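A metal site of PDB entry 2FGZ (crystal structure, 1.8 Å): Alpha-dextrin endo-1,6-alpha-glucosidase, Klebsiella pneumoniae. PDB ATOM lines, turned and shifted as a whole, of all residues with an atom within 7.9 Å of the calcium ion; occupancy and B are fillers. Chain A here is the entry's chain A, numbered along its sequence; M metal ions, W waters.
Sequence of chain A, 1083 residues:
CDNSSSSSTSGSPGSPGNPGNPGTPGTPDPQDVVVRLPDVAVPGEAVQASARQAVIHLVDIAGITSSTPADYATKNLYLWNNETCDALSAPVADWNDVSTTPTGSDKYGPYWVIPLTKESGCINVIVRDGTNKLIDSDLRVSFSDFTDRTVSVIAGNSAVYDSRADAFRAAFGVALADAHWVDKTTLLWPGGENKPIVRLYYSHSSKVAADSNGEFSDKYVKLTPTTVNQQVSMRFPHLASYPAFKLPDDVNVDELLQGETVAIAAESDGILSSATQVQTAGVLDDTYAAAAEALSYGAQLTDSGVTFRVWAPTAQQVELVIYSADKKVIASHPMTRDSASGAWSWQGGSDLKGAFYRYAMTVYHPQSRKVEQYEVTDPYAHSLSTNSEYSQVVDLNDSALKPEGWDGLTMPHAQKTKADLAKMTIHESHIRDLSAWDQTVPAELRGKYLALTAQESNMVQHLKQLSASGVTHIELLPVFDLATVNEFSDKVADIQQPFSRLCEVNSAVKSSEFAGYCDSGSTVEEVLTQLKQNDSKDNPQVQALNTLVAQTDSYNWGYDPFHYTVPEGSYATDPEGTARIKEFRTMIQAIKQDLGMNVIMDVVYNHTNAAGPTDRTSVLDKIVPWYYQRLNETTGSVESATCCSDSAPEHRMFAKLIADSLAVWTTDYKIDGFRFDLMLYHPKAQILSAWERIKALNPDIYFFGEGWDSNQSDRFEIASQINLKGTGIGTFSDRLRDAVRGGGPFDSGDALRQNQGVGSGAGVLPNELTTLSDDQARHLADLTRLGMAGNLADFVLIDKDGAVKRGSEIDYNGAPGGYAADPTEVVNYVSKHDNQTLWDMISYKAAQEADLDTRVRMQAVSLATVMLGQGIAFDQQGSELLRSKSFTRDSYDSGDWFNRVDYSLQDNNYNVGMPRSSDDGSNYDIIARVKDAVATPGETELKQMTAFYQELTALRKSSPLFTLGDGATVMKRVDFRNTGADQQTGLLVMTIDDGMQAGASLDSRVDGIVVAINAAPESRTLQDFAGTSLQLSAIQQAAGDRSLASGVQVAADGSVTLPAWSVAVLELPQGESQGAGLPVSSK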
ATOM      1  N   LEU A 384      14.057  -1.436 -15.738  1.00  0.00           N
ATOM      2  CA  LEU A 384      14.855  -2.359 -16.528  1.00  0.00           C
ATOM      3  C   LEU A 384      14.772  -3.804 -16.039  1.00  0.00           C
ATOM      4  O   LEU A 384      14.347  -4.064 -14.914  1.00  0.00           O
ATOM      5  CB  LEU A 384      16.336  -1.937 -16.465  1.00  0.00           C
ATOM      6  CG  LEU A 384      16.790  -0.574 -17.010  1.00  0.00           C
ATOM      7  CD1 LEU A 384      18.135  -0.177 -16.364  1.00  0.00           C
ATOM      8  CD2 LEU A 384      16.928  -0.661 -18.517  1.00  0.00           C
ATOM      9  N   SER A 385      15.183  -4.718 -16.901  1.00  0.00           N
ATOM     10  CA  SER A 385      15.219  -6.135 -16.557  1.00  0.00           C
ATOM     11  C   SER A 385      16.591  -6.333 -15.909  1.00  0.00           C
ATOM     12  O   SER A 385      17.387  -5.390 -15.840  1.00  0.00           O
ATOM     13  CB  SER A 385      15.131  -7.001 -17.814  1.00  0.00           C
ATOM     14  OG  SER A 385      16.294  -6.841 -18.616  1.00  0.00           O
ATOM     15  N   THR A 386      16.888  -7.533 -15.442  1.00  0.00           N
ATOM     16  CA  THR A 386      18.175  -7.798 -14.818  1.00  0.00           C
ATOM     17  C   THR A 386      19.355  -7.476 -15.729  1.00  0.00           C
ATOM     18  O   THR A 386      19.397  -7.891 -16.883  1.00  0.00           O
ATOM     19  CB  THR A 386      18.295  -9.277 -14.386  1.00  0.00           C
ATOM     20  OG1 THR A 386      17.231  -9.596 -13.479  1.00  0.00           O
ATOM     21  CG2 THR A 386      19.639  -9.528 -13.694  1.00  0.00           C
ATOM     22  N   ASN A 387      20.318  -6.736 -15.193  1.00  0.00           N
ATOM     23  CA  ASN A 387      21.537  -6.340 -15.915  1.00  0.00           C
ATOM     24  C   ASN A 387      21.259  -5.396 -17.081  1.00  0.00           C
ATOM     25  O   ASN A 387      22.069  -5.288 -18.007  1.00  0.00           O
ATOM     26  CB  ASN A 387      22.292  -7.576 -16.410  1.00  0.00           C
ATOM     27  CG  ASN A 387      23.796  -7.351 -16.468  1.00  0.00           C
ATOM     28  OD1 ASN A 387      24.483  -7.887 -17.347  1.00  0.00           O
ATOM     29  ND2 ASN A 387      24.322  -6.581 -15.525  1.00  0.00           N
ATOM     30  N   SER A 388      20.108  -4.730 -17.050  1.00  0.00           N
ATOM     31  CA  SER A 388      19.745  -3.736 -18.061  1.00  0.00           C
ATOM     32  C   SER A 388      19.591  -4.220 -19.504  1.00  0.00           C
ATOM     33  O   SER A 388      19.701  -3.415 -20.438  1.00  0.00           O
ATOM     34  CB  SER A 388      20.792  -2.615 -18.053  1.00  0.00           C
ATOM     35  OG  SER A 388      21.179  -2.295 -16.729  1.00  0.00           O
ATOM     36  N   PHE A 480      22.424   5.309  -9.791  1.00  0.00           N
ATOM     37  CA  PHE A 480      21.659   5.254 -11.036  1.00  0.00           C
ATOM     38  C   PHE A 480      22.214   3.960 -11.616  1.00  0.00           C
ATOM     39  O   PHE A 480      23.120   3.366 -11.017  1.00  0.00           O
ATOM     40  CB  PHE A 480      21.987   6.455 -11.938  1.00  0.00           C
ATOM     41  CG  PHE A 480      23.453   6.712 -12.077  1.00  0.00           C
ATOM     42  CD1 PHE A 480      24.205   6.027 -13.029  1.00  0.00           C
ATOM     43  CD2 PHE A 480      24.095   7.624 -11.241  1.00  0.00           C
ATOM     44  CE1 PHE A 480      25.576   6.239 -13.142  1.00  0.00           C
ATOM     45  CE2 PHE A 480      25.464   7.841 -11.340  1.00  0.00           C
ATOM     46  CZ  PHE A 480      26.210   7.154 -12.284  1.00  0.00           C
ATOM     47  N   ASP A 481      21.710   3.510 -12.762  1.00  0.00           N
ATOM     48  CA  ASP A 481      22.194   2.248 -13.330  1.00  0.00           C
ATOM     49  C   ASP A 481      23.616   2.259 -13.895  1.00  0.00           C
ATOM     50  O   ASP A 481      23.864   2.754 -14.986  1.00  0.00           O
ATOM     51  CB  ASP A 481      21.231   1.769 -14.417  1.00  0.00           C
ATOM     52  CG  ASP A 481      21.657   0.460 -15.035  1.00  0.00           C
ATOM     53  OD1 ASP A 481      22.153  -0.420 -14.299  1.00  0.00           O
ATOM     54  OD2 ASP A 481      21.487   0.289 -16.265  1.00  0.00           O
ATOM     55  N   LEU A 482      24.540   1.678 -13.127  1.00  0.00           N
ATOM     56  CA  LEU A 482      25.930   1.578 -13.557  1.00  0.00           C
ATOM     57  C   LEU A 482      26.087   0.294 -14.381  1.00  0.00           C
ATOM     58  O   LEU A 482      25.250  -0.595 -14.337  1.00  0.00           O
ATOM     59  CB  LEU A 482      26.862   1.557 -12.346  1.00  0.00           C
ATOM     60  CG  LEU A 482      26.578   0.538 -11.251  1.00  0.00           C
ATOM     61  CD1 LEU A 482      27.696  -0.492 -11.208  1.00  0.00           C
ATOM     62  CD2 LEU A 482      26.470   1.264  -9.903  1.00  0.00           C
ATOM     63  N   ALA A 483      27.186   0.196 -15.139  1.00  0.00           N
ATOM     64  CA  ALA A 483      27.399  -0.957 -15.992  1.00  0.00           C
ATOM     65  C   ALA A 483      28.444  -1.962 -15.518  1.00  0.00           C
ATOM     66  O   ALA A 483      28.391  -3.137 -15.877  1.00  0.00           O
ATOM     67  CB  ALA A 483      27.777  -0.476 -17.392  1.00  0.00           C
ATOM     68  N   THR A 484      29.375  -1.500 -14.681  1.00  0.00           N
ATOM     69  CA  THR A 484      30.484  -2.317 -14.200  1.00  0.00           C
ATOM     70  C   THR A 484      30.293  -3.376 -13.113  1.00  0.00           C
ATOM     71  O   THR A 484      31.261  -3.815 -12.489  1.00  0.00           O
ATOM     72  CB  THR A 484      31.628  -1.394 -13.784  1.00  0.00           C
ATOM     73  OG1 THR A 484      31.112  -0.331 -12.979  1.00  0.00           O
ATOM     74  CG2 THR A 484      32.286  -0.798 -15.029  1.00  0.00           C
ATOM     75  N   VAL A 485      29.052  -3.781 -12.904  1.00  0.00           N
ATOM     76  CA  VAL A 485      28.742  -4.849 -11.953  1.00  0.00           C
ATOM     77  C   VAL A 485      27.687  -5.696 -12.666  1.00  0.00           C
ATOM     78  O   VAL A 485      26.703  -5.151 -13.184  1.00  0.00           O
ATOM     79  CB  VAL A 485      28.148  -4.331 -10.627  1.00  0.00           C
ATOM     80  CG1 VAL A 485      27.608  -5.496  -9.811  1.00  0.00           C
ATOM     81  CG2 VAL A 485      29.211  -3.598  -9.826  1.00  0.00           C
ATOM     82  N   ASN A 486      27.897  -7.000 -12.712  1.00  0.00           N
ATOM     83  CA  ASN A 486      26.929  -7.880 -13.369  1.00  0.00           C
ATOM     84  C   ASN A 486      25.767  -8.082 -12.412  1.00  0.00           C
ATOM     85  O   ASN A 486      25.956  -8.508 -11.268  1.00  0.00           O
ATOM     86  CB  ASN A 486      27.575  -9.234 -13.705  1.00  0.00           C
ATOM     87  CG  ASN A 486      26.734 -10.038 -14.693  1.00  0.00           C
ATOM     88  OD1 ASN A 486      25.513 -10.113 -14.563  1.00  0.00           O
ATOM     89  ND2 ASN A 486      27.396 -10.654 -15.668  1.00  0.00           N
ATOM     90  N   GLU A 487      24.555  -7.774 -12.863  1.00  0.00           N
ATOM     91  CA  GLU A 487      23.376  -7.915 -12.016  1.00  0.00           C
ATOM     92  C   GLU A 487      22.822  -9.335 -11.970  1.00  0.00           C
ATOM     93  O   GLU A 487      21.875  -9.613 -11.235  1.00  0.00           O
ATOM     94  CB  GLU A 487      22.304  -6.912 -12.448  1.00  0.00           C
ATOM     95  CG  GLU A 487      22.833  -5.480 -12.418  1.00  0.00           C
ATOM     96  CD  GLU A 487      21.768  -4.439 -12.697  1.00  0.00           C
ATOM     97  OE1 GLU A 487      20.655  -4.817 -13.117  1.00  0.00           O
ATOM     98  OE2 GLU A 487      22.042  -3.228 -12.513  1.00  0.00           O
ATOM     99  N   ASP A 560      30.161   4.700 -14.141  1.00  0.00           N
ATOM    100  CA  ASP A 560      30.069   4.102 -15.460  1.00  0.00           C
ATOM    101  C   ASP A 560      28.589   4.025 -15.862  1.00  0.00           C
ATOM    102  O   ASP A 560      27.966   2.975 -15.760  1.00  0.00           O
ATOM    103  CB  ASP A 560      30.671   2.693 -15.425  1.00  0.00           C
ATOM    104  CG  ASP A 560      32.051   2.674 -14.794  1.00  0.00           C
ATOM    105  OD1 ASP A 560      32.212   2.158 -13.670  1.00  0.00           O
ATOM    106  OD2 ASP A 560      32.984   3.207 -15.439  1.00  0.00           O
ATOM    107  N   PHE A 562      25.095   3.489 -17.510  1.00  0.00           N
ATOM    108  CA  PHE A 562      24.483   2.576 -18.470  1.00  0.00           C
ATOM    109  C   PHE A 562      23.132   3.231 -18.799  1.00  0.00           C
ATOM    110  O   PHE A 562      22.789   3.422 -19.974  1.00  0.00           O
ATOM    111  CB  PHE A 562      24.293   1.185 -17.845  1.00  0.00           C
ATOM    112  CG  PHE A 562      24.081   0.082 -18.861  1.00  0.00           C
ATOM    113  CD1 PHE A 562      24.105  -1.255 -18.454  1.00  0.00           C
ATOM    114  CD2 PHE A 562      23.837   0.369 -20.197  1.00  0.00           C
ATOM    115  CE1 PHE A 562      23.895  -2.293 -19.371  1.00  0.00           C
ATOM    116  CE2 PHE A 562      23.622  -0.652 -21.127  1.00  0.00           C
ATOM    117  CZ  PHE A 562      23.651  -1.983 -20.714  1.00  0.00           C
ATOM    118  N   HIS A 563      22.364   3.555 -17.758  1.00  0.00           N
ATOM    119  CA  HIS A 563      21.069   4.243 -17.905  1.00  0.00           C
ATOM    120  C   HIS A 563      21.024   5.310 -16.815  1.00  0.00           C
ATOM    121  O   HIS A 563      21.150   5.010 -15.628  1.00  0.00           O
ATOM    122  CB  HIS A 563      19.908   3.267 -17.762  1.00  0.00           C
ATOM    123  CG  HIS A 563      19.881   2.213 -18.819  1.00  0.00           C
ATOM    124  ND1 HIS A 563      19.271   2.388 -20.046  1.00  0.00           N
ATOM    125  CD2 HIS A 563      20.475   0.997 -18.868  1.00  0.00           C
ATOM    126  CE1 HIS A 563      19.491   1.330 -20.801  1.00  0.00           C
ATOM    127  NE2 HIS A 563      20.218   0.466 -20.113  1.00  0.00           N
ATOM    128  N   VAL A 566      17.386   5.210 -14.013  1.00  0.00           N
ATOM    129  CA  VAL A 566      16.865   3.977 -13.441  1.00  0.00           C
ATOM    130  C   VAL A 566      17.820   3.640 -12.299  1.00  0.00           C
ATOM    131  O   VAL A 566      19.025   3.841 -12.440  1.00  0.00           O
ATOM    132  CB  VAL A 566      16.911   2.785 -14.425  1.00  0.00           C
ATOM    133  CG1 VAL A 566      16.162   1.589 -13.843  1.00  0.00           C
ATOM    134  CG2 VAL A 566      16.331   3.178 -15.776  1.00  0.00           C
ATOM    135  N   PRO A 567      17.306   3.170 -11.155  1.00  0.00           N
ATOM    136  CA  PRO A 567      18.201   2.840 -10.051  1.00  0.00           C
ATOM    137  C   PRO A 567      19.068   1.633 -10.440  1.00  0.00           C
ATOM    138  O   PRO A 567      18.671   0.836 -11.288  1.00  0.00           O
ATOM    139  CB  PRO A 567      17.242   2.488  -8.922  1.00  0.00           C
ATOM    140  CG  PRO A 567      16.029   3.323  -9.233  1.00  0.00           C
ATOM    141  CD  PRO A 567      15.897   3.145 -10.718  1.00  0.00           C
ATOM    142  N   GLU A 568      20.239   1.516  -9.815  1.00  0.00           N
ATOM    143  CA  GLU A 568      21.123   0.392 -10.087  1.00  0.00           C
ATOM    144  C   GLU A 568      20.431  -0.877  -9.596  1.00  0.00           C
ATOM    145  O   GLU A 568      19.766  -0.877  -8.554  1.00  0.00           O
ATOM    146  CB  GLU A 568      22.453   0.595  -9.352  1.00  0.00           C
ATOM    147  CG  GLU A 568      23.262  -0.685  -9.128  1.00  0.00           C
ATOM    148  CD  GLU A 568      23.700  -1.374 -10.416  1.00  0.00           C
ATOM    149  OE1 GLU A 568      24.238  -2.494 -10.315  1.00  0.00           O
ATOM    150  OE2 GLU A 568      23.532  -0.818 -11.524  1.00  0.00           O
ATOM    151  N   GLY A 569      20.586  -1.967 -10.347  1.00  0.00           N
ATOM    152  CA  GLY A 569      19.935  -3.215  -9.977  1.00  0.00           C
ATOM    153  C   GLY A 569      20.630  -4.107  -8.971  1.00  0.00           C
ATOM    154  O   GLY A 569      19.965  -4.778  -8.174  1.00  0.00           O
ATOM    155  N   SER A 570      21.959  -4.124  -8.972  1.00  0.00           N
ATOM    156  CA  SER A 570      22.696  -4.977  -8.041  1.00  0.00           C
ATOM    157  C   SER A 570      22.489  -4.598  -6.580  1.00  0.00           C
ATOM    158  O   SER A 570      22.714  -5.416  -5.690  1.00  0.00           O
ATOM    159  CB  SER A 570      24.194  -4.966  -8.375  1.00  0.00           C
ATOM    160  OG  SER A 570      24.785  -3.722  -8.050  1.00  0.00           O
ATOM    161  N   TYR A 571      22.054  -3.359  -6.328  1.00  0.00           N
ATOM    162  CA  TYR A 571      21.811  -2.915  -4.966  1.00  0.00           C
ATOM    163  C   TYR A 571      20.413  -3.284  -4.479  1.00  0.00           C
ATOM    164  O   TYR A 571      20.057  -3.013  -3.327  1.00  0.00           O
ATOM    165  CB  TYR A 571      22.022  -1.397  -4.832  1.00  0.00           C
ATOM    166  CG  TYR A 571      23.434  -0.941  -5.121  1.00  0.00           C
ATOM    167  CD1 TYR A 571      24.541  -1.703  -4.724  1.00  0.00           C
ATOM    168  CD2 TYR A 571      23.679   0.274  -5.768  1.00  0.00           C
ATOM    169  CE1 TYR A 571      25.837  -1.269  -4.959  1.00  0.00           C
ATOM    170  CE2 TYR A 571      24.981   0.724  -6.007  1.00  0.00           C
ATOM    171  CZ  TYR A 571      26.052  -0.062  -5.606  1.00  0.00           C
ATOM    172  OH  TYR A 571      27.337   0.364  -5.839  1.00  0.00           O
ATOM    173  N   ARG A 580      13.199  -2.933  -7.798  1.00  0.00           N
ATOM    174  CA  ARG A 580      14.212  -2.018  -7.297  1.00  0.00           C
ATOM    175  C   ARG A 580      13.721  -0.590  -7.050  1.00  0.00           C
ATOM    176  O   ARG A 580      14.276   0.143  -6.226  1.00  0.00           O
ATOM    177  CB  ARG A 580      15.387  -1.956  -8.276  1.00  0.00           C
ATOM    178  CG  ARG A 580      15.084  -1.157  -9.540  1.00  0.00           C
ATOM    179  CD  ARG A 580      16.258  -1.142 -10.505  1.00  0.00           C
ATOM    180  NE  ARG A 580      16.405  -2.396 -11.236  1.00  0.00           N
ATOM    181  CZ  ARG A 580      17.192  -2.558 -12.288  1.00  0.00           C
ATOM    182  NH1 ARG A 580      17.924  -1.533 -12.721  1.00  0.00           N
ATOM    183  NH2 ARG A 580      17.238  -3.709 -12.935  1.00  0.00           N
ATOM    184  N   ARG A 616      28.067  -3.640 -25.700  1.00  0.00           N
ATOM    185  CA  ARG A 616      26.844  -3.968 -24.992  1.00  0.00           C
ATOM    186  C   ARG A 616      26.234  -2.764 -24.278  1.00  0.00           C
ATOM    187  O   ARG A 616      25.023  -2.568 -24.292  1.00  0.00           O
ATOM    188  CB  ARG A 616      27.135  -5.070 -23.961  1.00  0.00           C
ATOM    189  CG  ARG A 616      26.000  -5.362 -22.988  1.00  0.00           C
ATOM    190  CD  ARG A 616      26.464  -6.325 -21.879  1.00  0.00           C
ATOM    191  NE  ARG A 616      27.492  -5.726 -21.031  1.00  0.00           N
ATOM    192  CZ  ARG A 616      27.265  -5.190 -19.823  1.00  0.00           C
ATOM    193  NH1 ARG A 616      26.036  -5.181 -19.326  1.00  0.00           N
ATOM    194  NH2 ARG A 616      28.263  -4.658 -19.128  1.00  0.00           N
HETATM  195 CA    CA M   1      23.562  -1.871 -13.483  1.00  0.00          CA
HETATM  196  O   HOH W   1      23.417  -3.138 -15.379  1.00  0.00           O
HETATM  197  O   HOH W   2      25.267  -2.989 -12.705  1.00  0.00           O
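The side-chain hydroxyl of Ser 388 sits at hydrogen-bond distance from the side-chain carboxylate of Asp 481 (2.6 Å). The backbone carbonyl oxygen (O) of Asp 481 is in hydrogen-bond range of the backbone NH (N) of Phe 562 (2.9 Å). N of His 563 is in hydrogen-bond range of O of Asp 481, at 3.3 Å. The backbone carbonyl oxygen (O) of Val 566 is in hydrogen-bond range of the backbone NH (N) of Asp 481 (2.7 Å). The side-chain carboxylate (OE1) of Glu 568 lies within hydrogen-bond range of the side-chain hydroxyl (OG) of Ser 570, at 2.6 Å. The side-chain carboxylate (OE2) of Glu 487 sits close to the backbone NH (N) of Gly 569. The side-chain carboxylate of Glu 487 is in hydrogen-bond range of the backbone NH of Asn 387. OE1 of Glu 487 lies within salt-bridge range of NH2 of Arg 580 (3.6 Å).
Within 4 Å of the calcium ion: Asp 481, Leu 482, Glu 487 and Glu 568.
The side-chain carboxylate (OD1) of Asp 481 binds the calcium ion (2.2 Å). Water W2 binds the calcium ion (2.2 Å). The side-chain carboxylate (OE2) of Glu 568 is bound to the calcium ion (2.2 Å). OE2 of Glu 487 binds the calcium ion, at 2.3 Å. The calcium ion is bound by the backbone carbonyl oxygen (O) of Leu 482 (2.3 Å). The calcium ion is bound by water W1, at 2.3 Å. The calcium ion has six donor atoms within binding distance.
Water W2 bridges the backbone carbonyl oxygen (O) of Val 485 and the side-chain carboxylate (OE1) of Glu 568.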
